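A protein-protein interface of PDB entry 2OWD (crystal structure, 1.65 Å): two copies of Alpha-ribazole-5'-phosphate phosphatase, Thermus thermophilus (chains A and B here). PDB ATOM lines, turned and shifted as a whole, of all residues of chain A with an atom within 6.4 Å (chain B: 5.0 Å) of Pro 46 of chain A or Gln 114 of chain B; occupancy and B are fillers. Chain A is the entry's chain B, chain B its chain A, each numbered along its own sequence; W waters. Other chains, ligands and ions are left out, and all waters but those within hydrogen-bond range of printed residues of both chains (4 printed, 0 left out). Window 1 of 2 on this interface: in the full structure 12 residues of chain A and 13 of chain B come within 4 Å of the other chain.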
ATOM      1  N   PRO A  43       7.973  -5.811 -13.518  1.00  0.00           N
ATOM      2  CA  PRO A  43       7.913  -5.920 -14.979  1.00  0.00           C
ATOM      3  C   PRO A  43       8.578  -7.221 -15.428  1.00  0.00           C
ATOM      4  O   PRO A  43       9.458  -7.735 -14.744  1.00  0.00           O
ATOM      5  CB  PRO A  43       8.678  -4.688 -15.448  1.00  0.00           C
ATOM      6  CG  PRO A  43       9.739  -4.541 -14.387  1.00  0.00           C
ATOM      7  CD  PRO A  43       8.942  -4.778 -13.106  1.00  0.00           C
ATOM      8  N   SER A  44       8.162  -7.742 -16.578  1.00  0.00           N
ATOM      9  CA  SER A  44       8.725  -8.988 -17.080  1.00  0.00           C
ATOM     10  C   SER A  44      10.036  -8.793 -17.841  1.00  0.00           C
ATOM     11  O   SER A  44      10.128  -9.079 -19.039  1.00  0.00           O
ATOM     12  CB  SER A  44       7.693  -9.704 -17.953  1.00  0.00           C
ATOM     13  OG  SER A  44       7.063  -8.793 -18.837  1.00  0.00           O
ATOM     14  N   LEU A  45      11.049  -8.305 -17.131  1.00  0.00           N
ATOM     15  CA  LEU A  45      12.375  -8.080 -17.707  1.00  0.00           C
ATOM     16  C   LEU A  45      13.222  -9.305 -17.399  1.00  0.00           C
ATOM     17  O   LEU A  45      12.835 -10.131 -16.577  1.00  0.00           O
ATOM     18  CB  LEU A  45      13.041  -6.869 -17.063  1.00  0.00           C
ATOM     19  CG  LEU A  45      12.239  -5.577 -16.928  1.00  0.00           C
ATOM     20  CD1 LEU A  45      13.150  -4.492 -16.388  1.00  0.00           C
ATOM     21  CD2 LEU A  45      11.666  -5.170 -18.285  1.00  0.00           C
ATOM     22  N   PRO A  46      14.382  -9.445 -18.068  1.00  0.00           N
ATOM     23  CA  PRO A  46      15.243 -10.599 -17.800  1.00  0.00           C
ATOM     24  C   PRO A  46      15.524 -10.597 -16.301  1.00  0.00           C
ATOM     25  O   PRO A  46      15.752  -9.536 -15.721  1.00  0.00           O
ATOM     26  CB  PRO A  46      16.490 -10.289 -18.622  1.00  0.00           C
ATOM     27  CG  PRO A  46      15.921  -9.578 -19.819  1.00  0.00           C
ATOM     28  CD  PRO A  46      14.917  -8.632 -19.176  1.00  0.00           C
ATOM     29  N   ALA A  47      15.512 -11.773 -15.677  1.00  0.00           N
ATOM     30  CA  ALA A  47      15.736 -11.865 -14.239  1.00  0.00           C
ATOM     31  C   ALA A  47      17.033 -12.547 -13.818  1.00  0.00           C
ATOM     32  O   ALA A  47      17.478 -13.522 -14.424  1.00  0.00           O
ATOM     33  CB  ALA A  47      14.550 -12.575 -13.568  1.00  0.00           C
ATOM     34  N   PHE A  48      17.618 -12.016 -12.753  1.00  0.00           N
ATOM     35  CA  PHE A  48      18.848 -12.534 -12.175  1.00  0.00           C
ATOM     36  C   PHE A  48      18.603 -12.604 -10.684  1.00  0.00           C
ATOM     37  O   PHE A  48      17.791 -11.851 -10.140  1.00  0.00           O
ATOM     38  CB  PHE A  48      20.012 -11.590 -12.453  1.00  0.00           C
ATOM     39  CG  PHE A  48      20.333 -11.442 -13.905  1.00  0.00           C
ATOM     40  CD1 PHE A  48      19.681 -10.491 -14.677  1.00  0.00           C
ATOM     41  CD2 PHE A  48      21.282 -12.260 -14.506  1.00  0.00           C
ATOM     42  CE1 PHE A  48      19.967 -10.351 -16.033  1.00  0.00           C
ATOM     43  CE2 PHE A  48      21.578 -12.131 -15.861  1.00  0.00           C
ATOM     44  CZ  PHE A  48      20.919 -11.174 -16.625  1.00  0.00           C
ATOM     45  N   PHE A  64       9.216 -15.541 -11.610  1.00  0.00           N
ATOM     46  CA  PHE A  64      10.427 -15.477 -12.436  1.00  0.00           C
ATOM     47  C   PHE A  64      11.263 -16.770 -12.376  1.00  0.00           C
ATOM     48  O   PHE A  64      11.142 -17.598 -11.457  1.00  0.00           O
ATOM     49  CB  PHE A  64      11.303 -14.304 -11.961  1.00  0.00           C
ATOM     50  CG  PHE A  64      10.656 -12.970 -12.233  1.00  0.00           C
ATOM     51  CD1 PHE A  64       9.788 -12.422 -11.294  1.00  0.00           C
ATOM     52  CD2 PHE A  64      10.986 -12.252 -13.375  1.00  0.00           C
ATOM     53  CE1 PHE A  64       9.231 -11.167 -11.513  1.00  0.00           C
ATOM     54  CE2 PHE A  64      10.422 -10.992 -13.585  1.00  0.00           C
ATOM     55  CZ  PHE A  64       9.542 -10.449 -12.659  1.00  0.00           C
ATOM     56  N   ARG A  67      18.518 -16.158 -13.760  1.00  0.00           N
ATOM     57  CA  ARG A  67      19.867 -16.691 -13.811  1.00  0.00           C
ATOM     58  C   ARG A  67      20.566 -16.460 -12.472  1.00  0.00           C
ATOM     59  O   ARG A  67      20.425 -15.419 -11.844  1.00  0.00           O
ATOM     60  CB  ARG A  67      20.627 -15.966 -14.922  1.00  0.00           C
ATOM     61  CG  ARG A  67      19.983 -16.160 -16.294  1.00  0.00           C
ATOM     62  CD  ARG A  67      20.514 -15.162 -17.328  1.00  0.00           C
ATOM     63  NE  ARG A  67      21.969 -15.281 -17.458  1.00  0.00           N
ATOM     64  CZ  ARG A  67      22.584 -14.437 -18.308  1.00  0.00           C
ATOM     65  NH1 ARG A  67      21.881 -13.543 -18.979  1.00  0.00           N
ATOM     66  NH2 ARG A  67      23.908 -14.514 -18.473  1.00  0.00           N
ATOM     67  N   LYS A 125      23.860  -6.162 -19.756  1.00  0.00           N
ATOM     68  CA  LYS A 125      23.709  -5.703 -21.134  1.00  0.00           C
ATOM     69  C   LYS A 125      22.291  -5.334 -21.548  1.00  0.00           C
ATOM     70  O   LYS A 125      22.047  -5.045 -22.717  1.00  0.00           O
ATOM     71  CB  LYS A 125      24.229  -6.765 -22.106  1.00  0.00           C
ATOM     72  CG  LYS A 125      25.632  -7.271 -21.813  1.00  0.00           C
ATOM     73  CD  LYS A 125      25.658  -8.758 -21.568  1.00  0.00           C
ATOM     74  CE  LYS A 125      25.687  -9.526 -22.885  1.00  0.00           C
ATOM     75  NZ  LYS A 125      24.387 -10.210 -23.142  1.00  0.00           N
ATOM     76  N   ALA A 126      21.358  -5.360 -20.606  1.00  0.00           N
ATOM     77  CA  ALA A 126      19.975  -5.009 -20.898  1.00  0.00           C
ATOM     78  C   ALA A 126      19.247  -4.825 -19.578  1.00  0.00           C
ATOM     79  O   ALA A 126      19.730  -5.266 -18.534  1.00  0.00           O
ATOM     80  CB  ALA A 126      19.304  -6.112 -21.713  1.00  0.00           C
ATOM     81  N   PRO A 127      18.084  -4.153 -19.606  1.00  0.00           N
ATOM     82  CA  PRO A 127      17.303  -3.928 -18.384  1.00  0.00           C
ATOM     83  C   PRO A 127      17.072  -5.263 -17.682  1.00  0.00           C
ATOM     84  O   PRO A 127      17.021  -6.306 -18.333  1.00  0.00           O
ATOM     85  CB  PRO A 127      16.011  -3.319 -18.918  1.00  0.00           C
ATOM     86  CG  PRO A 127      16.514  -2.512 -20.097  1.00  0.00           C
ATOM     87  CD  PRO A 127      17.445  -3.498 -20.764  1.00  0.00           C
ATOM     88  N   ALA A 128      16.909  -5.228 -16.365  1.00  0.00           N
ATOM     89  CA  ALA A 128      16.725  -6.459 -15.612  1.00  0.00           C
ATOM     90  C   ALA A 128      16.073  -6.271 -14.249  1.00  0.00           C
ATOM     91  O   ALA A 128      15.992  -5.165 -13.717  1.00  0.00           O
ATOM     92  CB  ALA A 128      18.084  -7.140 -15.418  1.00  0.00           C
ATOM     93  N   VAL A 129      15.609  -7.385 -13.704  1.00  0.00           N
ATOM     94  CA  VAL A 129      15.024  -7.437 -12.379  1.00  0.00           C
ATOM     95  C   VAL A 129      16.051  -8.275 -11.630  1.00  0.00           C
ATOM     96  O   VAL A 129      16.416  -9.368 -12.080  1.00  0.00           O
ATOM     97  CB  VAL A 129      13.675  -8.164 -12.376  1.00  0.00           C
ATOM     98  CG1 VAL A 129      13.175  -8.337 -10.937  1.00  0.00           C
ATOM     99  CG2 VAL A 129      12.670  -7.365 -13.186  1.00  0.00           C
ATOM    100  N   LEU A 130      16.522  -7.753 -10.501  1.00  0.00           N
ATOM    101  CA  LEU A 130      17.532  -8.431  -9.700  1.00  0.00           C
ATOM    102  C   LEU A 130      16.999  -8.800  -8.316  1.00  0.00           C
ATOM    103  O   LEU A 130      16.653  -7.927  -7.525  1.00  0.00           O
ATOM    104  CB  LEU A 130      18.757  -7.517  -9.547  1.00  0.00           C
ATOM    105  CG  LEU A 130      19.292  -6.876 -10.832  1.00  0.00           C
ATOM    106  CD1 LEU A 130      20.408  -5.893 -10.494  1.00  0.00           C
ATOM    107  CD2 LEU A 130      19.787  -7.957 -11.782  1.00  0.00           C
ATOM    108  N   PHE B  99       8.166 -16.146 -21.435  1.00  0.00           N
ATOM    109  CA  PHE B  99       9.533 -15.847 -21.892  1.00  0.00           C
ATOM    110  C   PHE B  99      10.577 -16.112 -20.802  1.00  0.00           C
ATOM    111  O   PHE B  99      11.422 -15.275 -20.526  1.00  0.00           O
ATOM    112  CB  PHE B  99       9.617 -14.386 -22.362  1.00  0.00           C
ATOM    113  CG  PHE B  99      10.568 -14.246 -23.533  1.00  0.00           C
ATOM    114  CD1 PHE B  99      10.243 -14.818 -24.759  1.00  0.00           C
ATOM    115  CD2 PHE B  99      11.727 -13.493 -23.407  1.00  0.00           C
ATOM    116  CE1 PHE B  99      11.089 -14.644 -25.857  1.00  0.00           C
ATOM    117  CE2 PHE B  99      12.570 -13.323 -24.512  1.00  0.00           C
ATOM    118  CZ  PHE B  99      12.253 -13.900 -25.731  1.00  0.00           C
ATOM    119  N   LEU B 110      16.463 -20.018 -23.199  1.00  0.00           N
ATOM    120  CA  LEU B 110      16.086 -18.627 -23.410  1.00  0.00           C
ATOM    121  C   LEU B 110      17.124 -17.684 -22.806  1.00  0.00           C
ATOM    122  O   LEU B 110      17.379 -16.610 -23.347  1.00  0.00           O
ATOM    123  CB  LEU B 110      14.703 -18.347 -22.821  1.00  0.00           C
ATOM    124  CG  LEU B 110      13.556 -18.374 -23.837  1.00  0.00           C
ATOM    125  CD1 LEU B 110      12.227 -18.141 -23.133  1.00  0.00           C
ATOM    126  CD2 LEU B 110      13.790 -17.289 -24.890  1.00  0.00           C
ATOM    127  N   SER B 111      17.724 -18.088 -21.690  1.00  0.00           N
ATOM    128  CA  SER B 111      18.754 -17.280 -21.038  1.00  0.00           C
ATOM    129  C   SER B 111      19.981 -17.156 -21.935  1.00  0.00           C
ATOM    130  O   SER B 111      20.575 -16.083 -22.051  1.00  0.00           O
ATOM    131  CB  SER B 111      19.164 -17.912 -19.703  1.00  0.00           C
ATOM    132  OG  SER B 111      18.113 -17.799 -18.764  1.00  0.00           O
ATOM    133  N   ALA B 112      20.366 -18.260 -22.568  1.00  0.00           N
ATOM    134  CA  ALA B 112      21.520 -18.246 -23.461  1.00  0.00           C
ATOM    135  C   ALA B 112      21.199 -17.387 -24.685  1.00  0.00           C
ATOM    136  O   ALA B 112      22.043 -16.648 -25.191  1.00  0.00           O
ATOM    137  CB  ALA B 112      21.862 -19.673 -23.894  1.00  0.00           C
ATOM    138  N   PHE B 113      19.965 -17.497 -25.154  1.00  0.00           N
ATOM    139  CA  PHE B 113      19.496 -16.745 -26.313  1.00  0.00           C
ATOM    140  C   PHE B 113      19.576 -15.246 -26.020  1.00  0.00           C
ATOM    141  O   PHE B 113      20.096 -14.473 -26.824  1.00  0.00           O
ATOM    142  CB  PHE B 113      18.055 -17.157 -26.618  1.00  0.00           C
ATOM    143  CG  PHE B 113      17.405 -16.371 -27.718  1.00  0.00           C
ATOM    144  CD1 PHE B 113      17.940 -16.359 -29.003  1.00  0.00           C
ATOM    145  CD2 PHE B 113      16.227 -15.675 -27.475  1.00  0.00           C
ATOM    146  CE1 PHE B 113      17.304 -15.665 -30.032  1.00  0.00           C
ATOM    147  CE2 PHE B 113      15.584 -14.978 -28.499  1.00  0.00           C
ATOM    148  CZ  PHE B 113      16.123 -14.974 -29.778  1.00  0.00           C
ATOM    149  N   GLN B 114      19.068 -14.843 -24.861  1.00  0.00           N
ATOM    150  CA  GLN B 114      19.089 -13.431 -24.482  1.00  0.00           C
ATOM    151  C   GLN B 114      20.519 -12.900 -24.399  1.00  0.00           C
ATOM    152  O   GLN B 114      20.811 -11.806 -24.882  1.00  0.00           O
ATOM    153  CB  GLN B 114      18.369 -13.236 -23.139  1.00  0.00           C
ATOM    154  CG  GLN B 114      16.845 -13.348 -23.244  1.00  0.00           C
ATOM    155  CD  GLN B 114      16.159 -13.397 -21.888  1.00  0.00           C
ATOM    156  OE1 GLN B 114      15.139 -12.743 -21.681  1.00  0.00           O
ATOM    157  NE2 GLN B 114      16.723 -14.164 -20.956  1.00  0.00           N
ATOM    158  N   GLU B 115      21.419 -13.676 -23.796  1.00  0.00           N
ATOM    159  CA  GLU B 115      22.807 -13.232 -23.667  1.00  0.00           C
ATOM    160  C   GLU B 115      23.413 -13.006 -25.044  1.00  0.00           C
ATOM    161  O   GLU B 115      24.105 -12.015 -25.282  1.00  0.00           O
ATOM    162  CB  GLU B 115      23.642 -14.269 -22.910  1.00  0.00           C
ATOM    163  CG  GLU B 115      25.049 -13.789 -22.578  1.00  0.00           C
ATOM    164  CD  GLU B 115      25.892 -14.860 -21.918  1.00  0.00           C
ATOM    165  OE1 GLU B 115      25.327 -15.691 -21.174  1.00  0.00           O
ATOM    166  OE2 GLU B 115      27.122 -14.867 -22.134  1.00  0.00           O
ATOM    167  N   ARG B 116      23.149 -13.941 -25.949  1.00  0.00           N
ATOM    168  CA  ARG B 116      23.651 -13.860 -27.314  1.00  0.00           C
ATOM    169  C   ARG B 116      23.136 -12.596 -28.006  1.00  0.00           C
ATOM    170  O   ARG B 116      23.905 -11.833 -28.591  1.00  0.00           O
ATOM    171  CB  ARG B 116      23.211 -15.109 -28.087  1.00  0.00           C
ATOM    172  CG  ARG B 116      23.346 -15.017 -29.585  1.00  0.00           C
ATOM    173  CD  ARG B 116      23.374 -16.402 -30.216  1.00  0.00           C
ATOM    174  NE  ARG B 116      22.097 -17.123 -30.257  1.00  0.00           N
ATOM    175  CZ  ARG B 116      21.098 -16.852 -31.093  1.00  0.00           C
ATOM    176  NH1 ARG B 116      21.194 -15.850 -31.955  1.00  0.00           N
ATOM    177  NH2 ARG B 116      20.029 -17.637 -31.129  1.00  0.00           N
ATOM    178  N   VAL B 117      21.830 -12.379 -27.935  1.00  0.00           N
ATOM    179  CA  VAL B 117      21.225 -11.212 -28.562  1.00  0.00           C
ATOM    180  C   VAL B 117      21.731  -9.897 -27.972  1.00  0.00           C
ATOM    181  O   VAL B 117      22.162  -9.005 -28.698  1.00  0.00           O
ATOM    182  CB  VAL B 117      19.680 -11.257 -28.435  1.00  0.00           C
ATOM    183  CG1 VAL B 117      19.074  -9.919 -28.854  1.00  0.00           C
ATOM    184  CG2 VAL B 117      19.130 -12.375 -29.308  1.00  0.00           C
ATOM    185  N   PHE B 118      21.685  -9.775 -26.651  1.00  0.00           N
ATOM    186  CA  PHE B 118      22.108  -8.536 -26.014  1.00  0.00           C
ATOM    187  C   PHE B 118      23.595  -8.267 -26.155  1.00  0.00           C
ATOM    188  O   PHE B 118      24.021  -7.117 -26.180  1.00  0.00           O
ATOM    189  CB  PHE B 118      21.687  -8.542 -24.544  1.00  0.00           C
ATOM    190  CG  PHE B 118      20.205  -8.726 -24.350  1.00  0.00           C
ATOM    191  CD1 PHE B 118      19.307  -8.266 -25.309  1.00  0.00           C
ATOM    192  CD2 PHE B 118      19.707  -9.349 -23.212  1.00  0.00           C
ATOM    193  CE1 PHE B 118      17.926  -8.425 -25.136  1.00  0.00           C
ATOM    194  CE2 PHE B 118      18.327  -9.511 -23.029  1.00  0.00           C
ATOM    195  CZ  PHE B 118      17.440  -9.047 -23.994  1.00  0.00           C
ATOM    196  N   ARG B 119      24.386  -9.330 -26.256  1.00  0.00           N
ATOM    197  CA  ARG B 119      25.821  -9.168 -26.427  1.00  0.00           C
ATOM    198  C   ARG B 119      26.080  -8.590 -27.815  1.00  0.00           C
ATOM    199  O   ARG B 119      26.956  -7.741 -27.997  1.00  0.00           O
ATOM    200  CB  ARG B 119      26.531 -10.517 -26.276  1.00  0.00           C
ATOM    201  CG  ARG B 119      28.035 -10.434 -26.434  1.00  0.00           C
ATOM    202  CD  ARG B 119      28.718 -11.651 -25.837  1.00  0.00           C
ATOM    203  NE  ARG B 119      28.404 -11.787 -24.417  1.00  0.00           N
ATOM    204  CZ  ARG B 119      29.030 -12.615 -23.585  1.00  0.00           C
ATOM    205  NH1 ARG B 119      30.011 -13.390 -24.030  1.00  0.00           N
ATOM    206  NH2 ARG B 119      28.678 -12.663 -22.308  1.00  0.00           N
ATOM    207  N   ALA B 139      12.640 -10.480 -27.620  1.00  0.00           N
ATOM    208  CA  ALA B 139      13.576 -10.368 -26.500  1.00  0.00           C
ATOM    209  C   ALA B 139      13.887  -8.901 -26.214  1.00  0.00           C
ATOM    210  O   ALA B 139      13.939  -8.470 -25.057  1.00  0.00           O
ATOM    211  CB  ALA B 139      14.861 -11.121 -26.818  1.00  0.00           C
ATOM    212  N   ALA B 143      12.514  -6.667 -22.953  1.00  0.00           N
ATOM    213  CA  ALA B 143      13.518  -6.081 -22.074  1.00  0.00           C
ATOM    214  C   ALA B 143      13.225  -4.600 -21.860  1.00  0.00           C
ATOM    215  O   ALA B 143      13.606  -4.000 -20.863  1.00  0.00           O
ATOM    216  CB  ALA B 143      14.901  -6.259 -22.707  1.00  0.00           C
HETATM  217  O   HOH W   1      22.807 -16.656 -20.381  1.00  0.00           O
HETATM  218  O   HOH W   2      23.251  -4.763 -25.019  1.00  0.00           O
HETATM  219  O   HOH W   3      18.834 -13.230 -19.391  1.00  0.00           O
HETATM  220  O   HOH W   4      25.567 -17.164 -18.664  1.00  0.00           O
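NZ of Lys 125 of chain A sits close to N of Arg 119 of chain B (3.2 Å).
The backbone carbonyl oxygen (O) of Glu 115 of chain B lies within hydrogen-bond range of the side-chain amino group (NZ) of Lys 125 of chain A.
The side-chain carboxylate (OE1) of Glu 115 of chain B is in salt-bridge range of the guanidinium group (NH2) of Arg 67 of chain A (3.3 Å).
The guanidinium group of Arg 119 of chain B is in salt-bridge range of the side-chain carboxylate of Glu 115 of chain B.
O of Ala 47 of chain A lies within hydrogen-bond range of N of Arg 67 of chain A, 2.9 Å away.
The backbone carbonyl oxygen (O) of Pro 46 of chain A lies within hydrogen-bond range of the backbone NH (N) of Val 129 of chain A (3.0 Å).
O of Leu 110 of chain B lies close to NE2 of Gln 114 of chain B, at 3.5 Å.
Leu 45 of chain A touches Ala 143 of chain B.
Pro 46 of chain A touches Gln 114 of chain B.
Arg 67 of chain A touches Ser 111 of chain B.
Lys 125 of chain A touches Phe 118 of chain B.
Ala 126 of chain A touches Phe 118 of chain B (CB to CD2, 3.6 Å).
Pro 127 of chain A touches Ala 143 of chain B (CB to O, 3.2 Å).
Printed residues of chain B within 4 Å of Leu 45 of chain A: Ala 143.
Of the printed residues of chain B, Pro 46 of chain A touches Gln 114 (3.8 Å).
Of the printed residues of chain B, Pro 127 of chain A touches Ala 143.
Phe 113 of chain B touches none of the printed residues of chain A.
Gln 114 of chain B touches just one residue of chain A: Pro 46 (3.8 Å).
Of the printed residues of chain A, Glu 115 of chain B touches Arg 67 (3.3 Å) and Lys 125 (2.8 Å).
Of the printed residues of chain A, Ala 143 of chain B touches Leu 45 (3.4 Å) and Pro 127 (3.2 Å).
The nearest printed residue of chain B that does not touch Pro 46 of chain A is Phe 118 of chain B (4.01 Å).
The nearest residue of chain A that does not touch Gln 114 of chain B is Lys 125 of chain A (4.3 Å).
Of the 13 printed residues of chain B, 6 touch a printed residue of chain A.
Hydrophobic or aromatic side chains of chain B within 4 Å of the printed part of chain A: Phe 118.
Along chain A the printed residues that touch a printed residue of chain B span positions 45 to 127.
Among the printed residues, Asp or Glu carboxylates within 4 Å of a Lys or Arg side-chain nitrogen of the other chain: Arg 67 of chain A with Glu 115 of chain B (3.3 Å).
No position is printed for both chains.
Water W2 lies within hydrogen-bond range of O of Lys 125 of chain A and O of Phe 118 of chain B.
Water W3 lies within hydrogen-bond range of NE2 of Gln 114 of chain B (2.8 Å) and NH1 of Arg 67 of chain A (3.1 Å).
Water W1 lies within hydrogen-bond range of the side-chain carboxylate (OE1) of Glu 115 of chain B (2.8 Å), the backbone carbonyl oxygen (O) of Ser 111 of chain B (2.8 Å) and the guanidinium group (NH2) of Arg 67 of chain A (3.1 Å).
Water W4 bridges the side-chain carboxylate (OE1) of Glu 115 of chain B (2.9 Å) and the guanidinium group (NH2) of Arg 67 of chain A (3.1 Å).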
